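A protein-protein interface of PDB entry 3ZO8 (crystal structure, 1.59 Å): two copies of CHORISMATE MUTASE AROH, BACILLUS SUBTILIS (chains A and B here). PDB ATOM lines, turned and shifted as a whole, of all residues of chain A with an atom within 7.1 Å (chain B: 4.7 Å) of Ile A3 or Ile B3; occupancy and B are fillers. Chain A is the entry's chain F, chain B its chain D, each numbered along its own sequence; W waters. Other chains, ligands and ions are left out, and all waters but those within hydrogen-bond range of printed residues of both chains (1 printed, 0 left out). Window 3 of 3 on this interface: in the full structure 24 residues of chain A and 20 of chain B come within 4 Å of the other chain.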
ATOM      1  N   MET A   1       4.611 -10.439  -3.525  1.00  0.00           N
ATOM      2  CA  MET A   1       4.996 -11.340  -2.400  1.00  0.00           C
ATOM      3  C   MET A   1       3.876 -11.395  -1.371  1.00  0.00           C
ATOM      4  O   MET A   1       3.146 -10.422  -1.191  1.00  0.00           O
ATOM      5  CB  MET A   1       6.284 -10.842  -1.743  1.00  0.00           C
ATOM      6  CG  MET A   1       6.976 -11.874  -0.867  1.00  0.00           C
ATOM      7  SD  MET A   1       8.615 -11.349  -0.325  1.00  0.00           S
ATOM      8  CE  MET A   1       9.352 -10.874  -1.887  1.00  0.00           C
ATOM      9  N   MET A   2       3.729 -12.535  -0.704  1.00  0.00           N
ATOM     10  CA  MET A   2       2.720 -12.647   0.340  1.00  0.00           C
ATOM     11  C   MET A   2       2.980 -11.585   1.397  1.00  0.00           C
ATOM     12  O   MET A   2       4.109 -11.113   1.564  1.00  0.00           O
ATOM     13  CB  MET A   2       2.712 -14.049   0.962  1.00  0.00           C
ATOM     14  CG  MET A   2       1.677 -14.264   2.066  1.00  0.00           C
ATOM     15  SD  MET A   2      -0.044 -13.878   1.654  1.00  0.00           S
ATOM     16  CE  MET A   2      -0.905 -14.738   2.967  1.00  0.00           C
ATOM     17  N   ILE A   3       1.910 -11.188   2.075  1.00  0.00           N
ATOM     18  CA  ILE A   3       1.984 -10.299   3.222  1.00  0.00           C
ATOM     19  C   ILE A   3       1.675 -11.099   4.499  1.00  0.00           C
ATOM     20  O   ILE A   3       0.871 -12.034   4.469  1.00  0.00           O
ATOM     21  CB  ILE A   3       0.982  -9.132   3.058  1.00  0.00           C
ATOM     22  CG1 ILE A   3       1.192  -8.446   1.704  1.00  0.00           C
ATOM     23  CG2 ILE A   3       1.095  -8.141   4.208  1.00  0.00           C
ATOM     24  CD1 ILE A   3       2.466  -7.645   1.606  1.00  0.00           C
ATOM     25  N   ARG A   4       2.320 -10.735   5.609  1.00  0.00           N
ATOM     26  CA  ARG A   4       2.127 -11.422   6.895  1.00  0.00           C
ATOM     27  C   ARG A   4       2.216 -10.481   8.114  1.00  0.00           C
ATOM     28  O   ARG A   4       3.005  -9.527   8.132  1.00  0.00           O
ATOM     29  CB  ARG A   4       3.137 -12.573   7.051  1.00  0.00           C
ATOM     30  CG  ARG A   4       3.086 -13.634   5.954  1.00  0.00           C
ATOM     31  CD  ARG A   4       2.678 -15.012   6.465  1.00  0.00           C
ATOM     32  NE  ARG A   4       2.466 -15.950   5.362  1.00  0.00           N
ATOM     33  CZ  ARG A   4       1.296 -16.516   5.071  1.00  0.00           C
ATOM     34  NH1 ARG A   4       0.224 -16.263   5.812  1.00  0.00           N
ATOM     35  NH2 ARG A   4       1.200 -17.344   4.044  1.00  0.00           N
ATOM     36  N   GLY A   5       1.399 -10.761   9.127  1.00  0.00           N
ATOM     37  CA  GLY A   5       1.462 -10.062  10.409  1.00  0.00           C
ATOM     38  C   GLY A   5       2.480 -10.624  11.397  1.00  0.00           C
ATOM     39  O   GLY A   5       2.653 -11.852  11.521  1.00  0.00           O
ATOM     40  N   GLU A  40      11.373  -1.002   4.162  1.00  0.00           N
ATOM     41  CA  GLU A  40      10.608  -0.822   2.920  1.00  0.00           C
ATOM     42  C   GLU A  40       9.627  -1.981   2.627  1.00  0.00           C
ATOM     43  O   GLU A  40       8.739  -1.873   1.777  1.00  0.00           O
ATOM     44  CB  GLU A  40      11.563  -0.596   1.739  1.00  0.00           C
ATOM     45  CG  GLU A  40      12.472  -1.777   1.433  1.00  0.00           C
ATOM     46  CD  GLU A  40      13.839  -1.687   2.098  1.00  0.00           C
ATOM     47  OE1 GLU A  40      14.027  -0.861   3.023  1.00  0.00           O
ATOM     48  OE2 GLU A  40      14.735  -2.458   1.686  1.00  0.00           O
ATOM     49  N   ASP A  41       9.783  -3.085   3.345  1.00  0.00           N
ATOM     50  CA  ASP A  41       8.910  -4.230   3.165  1.00  0.00           C
ATOM     51  C   ASP A  41       7.806  -4.211   4.220  1.00  0.00           C
ATOM     52  O   ASP A  41       6.965  -5.112   4.266  1.00  0.00           O
ATOM     53  CB  ASP A  41       9.715  -5.532   3.256  1.00  0.00           C
ATOM     54  CG  ASP A  41      10.806  -5.647   2.174  1.00  0.00           C
ATOM     55  OD1 ASP A  41      10.623  -5.148   1.035  1.00  0.00           O
ATOM     56  OD2 ASP A  41      11.852  -6.265   2.460  1.00  0.00           O
ATOM     57  N   VAL A  42       7.835  -3.195   5.081  1.00  0.00           N
ATOM     58  CA  VAL A  42       6.806  -3.019   6.112  1.00  0.00           C
ATOM     59  C   VAL A  42       5.633  -2.239   5.530  1.00  0.00           C
ATOM     60  O   VAL A  42       5.763  -1.052   5.185  1.00  0.00           O
ATOM     61  CB  VAL A  42       7.335  -2.319   7.394  1.00  0.00           C
ATOM     62  CG1 VAL A  42       6.203  -2.070   8.381  1.00  0.00           C
ATOM     63  CG2 VAL A  42       8.422  -3.161   8.046  1.00  0.00           C
ATOM     64  N   VAL A  43       4.503  -2.929   5.403  1.00  0.00           N
ATOM     65  CA  VAL A  43       3.255  -2.338   4.938  1.00  0.00           C
ATOM     66  C   VAL A  43       2.791  -1.236   5.887  1.00  0.00           C
ATOM     67  O   VAL A  43       2.546  -0.103   5.459  1.00  0.00           O
ATOM     68  CB  VAL A  43       2.153  -3.415   4.831  1.00  0.00           C
ATOM     69  CG1 VAL A  43       0.815  -2.786   4.487  1.00  0.00           C
ATOM     70  CG2 VAL A  43       2.543  -4.478   3.813  1.00  0.00           C
ATOM     71  N   GLN A  44       2.667  -1.584   7.172  1.00  0.00           N
ATOM     72  CA  GLN A  44       2.216  -0.657   8.204  1.00  0.00           C
ATOM     73  C   GLN A  44       2.355  -1.330   9.557  1.00  0.00           C
ATOM     74  O   GLN A  44       2.600  -2.539   9.630  1.00  0.00           O
ATOM     75  CB  GLN A  44       0.750  -0.285   7.998  1.00  0.00           C
ATOM     76  CG  GLN A  44      -0.218  -1.392   8.391  1.00  0.00           C
ATOM     77  CD  GLN A  44      -1.580  -1.239   7.741  1.00  0.00           C
ATOM     78  OE1 GLN A  44      -1.687  -0.791   6.602  1.00  0.00           O
ATOM     79  NE2 GLN A  44      -2.631  -1.602   8.467  1.00  0.00           N
ATOM     80  N   THR A  94       2.865  -5.426   9.810  1.00  0.00           N
ATOM     81  CA  THR A  94       2.434  -6.104   8.601  1.00  0.00           C
ATOM     82  C   THR A  94       3.558  -5.943   7.588  1.00  0.00           C
ATOM     83  O   THR A  94       4.011  -4.819   7.336  1.00  0.00           O
ATOM     84  CB  THR A  94       1.119  -5.491   8.073  1.00  0.00           C
ATOM     85  OG1 THR A  94       0.216  -5.278   9.166  1.00  0.00           O
ATOM     86  CG2 THR A  94       0.452  -6.412   7.074  1.00  0.00           C
ATOM     87  N   VAL A  95       4.024  -7.065   7.042  1.00  0.00           N
ATOM     88  CA  VAL A  95       5.249  -7.094   6.230  1.00  0.00           C
ATOM     89  C   VAL A  95       5.118  -7.996   5.010  1.00  0.00           C
ATOM     90  O   VAL A  95       4.439  -9.027   5.055  1.00  0.00           O
ATOM     91  CB  VAL A  95       6.487  -7.599   7.027  1.00  0.00           C
ATOM     92  CG1 VAL A  95       6.687  -6.818   8.326  1.00  0.00           C
ATOM     93  CG2 VAL A  95       6.402  -9.098   7.292  1.00  0.00           C
ATOM     94  N   GLN A  96       5.788  -7.604   3.928  1.00  0.00           N
ATOM     95  CA  GLN A  96       5.988  -8.474   2.779  1.00  0.00           C
ATOM     96  C   GLN A  96       7.067  -9.508   3.102  1.00  0.00           C
ATOM     97  O   GLN A  96       8.165  -9.157   3.549  1.00  0.00           O
ATOM     98  CB  GLN A  96       6.392  -7.654   1.553  1.00  0.00           C
ATOM     99  CG  GLN A  96       6.514  -8.472   0.281  1.00  0.00           C
ATOM    100  CD  GLN A  96       6.813  -7.617  -0.937  1.00  0.00           C
ATOM    101  OE1 GLN A  96       6.055  -7.615  -1.908  1.00  0.00           O
ATOM    102  NE2 GLN A  96       7.916  -6.877  -0.887  1.00  0.00           N
ATOM    103  N   THR A  97       6.750 -10.785   2.891  1.00  0.00           N
ATOM    104  CA  THR A  97       7.707 -11.855   3.164  1.00  0.00           C
ATOM    105  C   THR A  97       7.336 -13.172   2.489  1.00  0.00           C
ATOM    106  O   THR A  97       6.160 -13.434   2.228  1.00  0.00           O
ATOM    107  CB  THR A  97       7.870 -12.095   4.680  1.00  0.00           C
ATOM    108  OG1 THR A  97       8.816 -13.148   4.900  1.00  0.00           O
ATOM    109  CG2 THR A  97       6.536 -12.478   5.312  1.00  0.00           C
ATOM    110  N   ASP A  98       8.346 -13.993   2.207  1.00  0.00           N
ATOM    111  CA  ASP A  98       8.116 -15.352   1.717  1.00  0.00           C
ATOM    112  C   ASP A  98       8.251 -16.396   2.834  1.00  0.00           C
ATOM    113  O   ASP A  98       8.013 -17.580   2.613  1.00  0.00           O
ATOM    114  CB  ASP A  98       9.002 -15.694   0.504  1.00  0.00           C
ATOM    115  CG  ASP A  98      10.489 -15.566   0.794  1.00  0.00           C
ATOM    116  OD1 ASP A  98      10.857 -14.994   1.843  1.00  0.00           O
ATOM    117  OD2 ASP A  98      11.294 -16.035  -0.044  1.00  0.00           O
ATOM    118  N   MET B   2       3.168  -3.829  -4.457  1.00  0.00           N
ATOM    119  CA  MET B   2       3.287  -3.899  -3.003  1.00  0.00           C
ATOM    120  C   MET B   2       2.026  -3.371  -2.327  1.00  0.00           C
ATOM    121  O   MET B   2       1.170  -2.775  -2.975  1.00  0.00           O
ATOM    122  CB  MET B   2       4.546  -3.145  -2.550  1.00  0.00           C
ATOM    123  CG  MET B   2       4.836  -3.122  -1.054  1.00  0.00           C
ATOM    124  SD  MET B   2       4.906  -4.673  -0.120  1.00  0.00           S
ATOM    125  CE  MET B   2       5.219  -4.002   1.507  1.00  0.00           C
ATOM    126  N   ILE B   3       1.890  -3.641  -1.033  1.00  0.00           N
ATOM    127  CA  ILE B   3       0.811  -3.078  -0.232  1.00  0.00           C
ATOM    128  C   ILE B   3       1.401  -2.019   0.701  1.00  0.00           C
ATOM    129  O   ILE B   3       2.437  -2.246   1.315  1.00  0.00           O
ATOM    130  CB  ILE B   3       0.118  -4.158   0.623  1.00  0.00           C
ATOM    131  CG1 ILE B   3      -0.301  -5.371  -0.229  1.00  0.00           C
ATOM    132  CG2 ILE B   3      -1.041  -3.559   1.405  1.00  0.00           C
ATOM    133  CD1 ILE B   3      -1.112  -5.054  -1.468  1.00  0.00           C
ATOM    134  N   ARG B   4       0.753  -0.865   0.804  1.00  0.00           N
ATOM    135  CA  ARG B   4       1.258   0.205   1.661  1.00  0.00           C
ATOM    136  C   ARG B   4       0.148   0.877   2.452  1.00  0.00           C
ATOM    137  O   ARG B   4      -0.973   1.024   1.968  1.00  0.00           O
ATOM    138  CB  ARG B   4       1.985   1.265   0.833  1.00  0.00           C
ATOM    139  CG  ARG B   4       3.110   0.722  -0.031  1.00  0.00           C
ATOM    140  CD  ARG B   4       4.479   1.230   0.383  1.00  0.00           C
ATOM    141  NE  ARG B   4       5.532   0.518  -0.337  1.00  0.00           N
ATOM    142  CZ  ARG B   4       6.432  -0.268   0.243  1.00  0.00           C
ATOM    143  NH1 ARG B   4       6.430  -0.426   1.564  1.00  0.00           N
ATOM    144  NH2 ARG B   4       7.343  -0.887  -0.496  1.00  0.00           N
ATOM    145  N   GLY B   5       0.476   1.287   3.672  1.00  0.00           N
ATOM    146  CA  GLY B   5      -0.437   2.067   4.494  1.00  0.00           C
ATOM    147  C   GLY B   5      -0.305   3.557   4.234  1.00  0.00           C
ATOM    148  O   GLY B   5       0.802   4.080   4.098  1.00  0.00           O
ATOM    149  N   VAL B  43      -7.252  -2.358   0.348  1.00  0.00           N
ATOM    150  CA  VAL B  43      -7.392  -3.605   1.092  1.00  0.00           C
ATOM    151  C   VAL B  43      -8.416  -3.455   2.203  1.00  0.00           C
ATOM    152  O   VAL B  43      -9.315  -4.272   2.346  1.00  0.00           O
ATOM    153  CB  VAL B  43      -6.047  -4.043   1.698  1.00  0.00           C
ATOM    154  CG1 VAL B  43      -6.195  -5.353   2.458  1.00  0.00           C
ATOM    155  CG2 VAL B  43      -5.012  -4.180   0.598  1.00  0.00           C
ATOM    156  N   THR B  94      -5.032   1.055   3.842  1.00  0.00           N
ATOM    157  CA  THR B  94      -4.094   0.093   3.277  1.00  0.00           C
ATOM    158  C   THR B  94      -4.447  -0.126   1.812  1.00  0.00           C
ATOM    159  O   THR B  94      -5.572  -0.523   1.491  1.00  0.00           O
ATOM    160  CB  THR B  94      -4.141  -1.248   4.037  1.00  0.00           C
ATOM    161  OG1 THR B  94      -4.035  -1.002   5.447  1.00  0.00           O
ATOM    162  CG2 THR B  94      -3.008  -2.178   3.574  1.00  0.00           C
ATOM    163  N   VAL B  95      -3.497   0.171   0.929  1.00  0.00           N
ATOM    164  CA  VAL B  95      -3.728   0.064  -0.510  1.00  0.00           C
ATOM    165  C   VAL B  95      -2.649  -0.750  -1.224  1.00  0.00           C
ATOM    166  O   VAL B  95      -1.503  -0.795  -0.780  1.00  0.00           O
ATOM    167  CB  VAL B  95      -3.792   1.465  -1.164  1.00  0.00           C
ATOM    168  CG1 VAL B  95      -4.792   2.358  -0.439  1.00  0.00           C
ATOM    169  CG2 VAL B  95      -2.412   2.109  -1.197  1.00  0.00           C
ATOM    170  N   GLN B  96      -3.026  -1.400  -2.327  1.00  0.00           N
ATOM    171  CA  GLN B  96      -2.060  -1.928  -3.301  1.00  0.00           C
ATOM    172  C   GLN B  96      -1.525  -0.792  -4.163  1.00  0.00           C
ATOM    173  O   GLN B  96      -2.297  -0.043  -4.776  1.00  0.00           O
ATOM    174  CB  GLN B  96      -2.716  -2.977  -4.207  1.00  0.00           C
ATOM    175  CG  GLN B  96      -1.726  -3.737  -5.088  1.00  0.00           C
ATOM    176  CD  GLN B  96      -2.396  -4.804  -5.939  1.00  0.00           C
ATOM    177  OE1 GLN B  96      -1.961  -5.956  -5.967  1.00  0.00           O
ATOM    178  NE2 GLN B  96      -3.463  -4.428  -6.628  1.00  0.00           N
HETATM  179  O   HOH W   1       4.943   0.944   3.541  1.00  0.00           O
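Ile A3 touches just one residue of chain B: Ile B3.
Arg A4 touches none of the printed residues of chain B.
Gly A5 touches none of the printed residues of chain B.
Printed residues of chain B within 4 Å of Glu A40: Arg B4 (2.7 Å).
Of chain A, only Ile A3 and Val A43 come within 4 Å of Ile B3.
Of the printed residues of chain A, Arg B4 touches Glu A40, Val A42 and Val A43.
Printed residues of chain A within 4 Å of Thr B94: Val A43 (3.98 Å) and Gln A44 (2.6 Å).
The nearest residue of chain B that does not touch Ile A3 is Met B2 (4.2 Å).
The nearest printed residue of chain A that does not touch Met B2 is Glu A40 (4.1 Å).
NH1 of Arg B4 is in hydrogen-bond range of O of Glu A40 (2.7 Å).
OG1 of Thr B94 lies within hydrogen-bond range of OE1 of Gln A44 (2.6 Å).
The side-chain amide oxygen (OE1) of Gln A96 sits close to the side-chain sulfur (SD) of Met B2.
The backbone carbonyl oxygen (O) of Val A43 sits at hydrogen-bond distance from the backbone NH (N) of Gly B5 (3.1 Å).
Printed residues of chain B that touch a printed residue of chain A: Met B2, Ile B3, Arg B4, Gly B5 and Thr B94.
Hydrophobic or aromatic side chains of chain B within 4 Å of the printed part of chain A: Met B2 and Ile B3.
Along chain B the printed residues that touch a printed residue of chain A span positions 2 to 94.
Among the printed residues, 12 pairs touch across the chains.
Among the printed residues, no Asp or Glu carboxylate lies within 4 Å of a Lys or Arg side-chain nitrogen of the other chain.
The backbone carbonyl oxygen (O) of Asp A41 is in hydrogen-bond range of the backbone NH (N) of Gln A96 (2.8 Å).
The backbone NH (N) of Arg B4 sits at hydrogen-bond distance from the backbone carbonyl oxygen (O) of Val B95.
The backbone NH (N) of Val A43 sits at hydrogen-bond distance from the backbone carbonyl oxygen (O) of Thr A94, at 2.7 Å.
The backbone carbonyl oxygen (O) of Thr B94 is in hydrogen-bond range of the backbone NH (N) of Val B43, at 2.7 Å.
The backbone carbonyl oxygen of Gln A44 sits at hydrogen-bond distance from the backbone NH of Thr A94, 2.9 Å away.
Ile B3 touches Ile A3 (CG1 to CG1, 3.9 Å).
CE of Met B2 touches O of Asp A41, at 3.4 Å.
Arg B4 touches Val A42 (NH1 to O, 3.7 Å).
Val A43 touches Met B2 (CG2 to CE, 3.6 Å).
CG2 of Val A43 touches O of Ile B3, 3.4 Å away.
O of Val A43 touches C of Arg B4, 3.97 Å away.
CG1 of Val A43 touches CG2 of Thr B94 (3.98 Å).
Gly B5 touches Gln A44.
Ile B3 touches its own counterpart, Ile A3.
Val A43 touches Met B2, but with the chains exchanged Met A2 does not touch Val B43 (10.5 Å).
Val A43 touches Ile B3, but with the chains exchanged Ile A3 does not touch Val B43 (7.6 Å).
Val A43 touches Arg B4, but with the chains exchanged Arg A4 does not touch Val B43 (10.6 Å).
Positions printed for both chains: 2, 3, 4, 5, 43, 94, 95 and 96.
Of the 12 pairs that touch across the chains among the printed residues, 1 has its exchanged pair printed and touching as well.
Water W1 lies within hydrogen-bond range of O of Val A42 (2.7 Å), NH1 of Arg B4 (2.8 Å) and O of Val A43 (3.2 Å).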
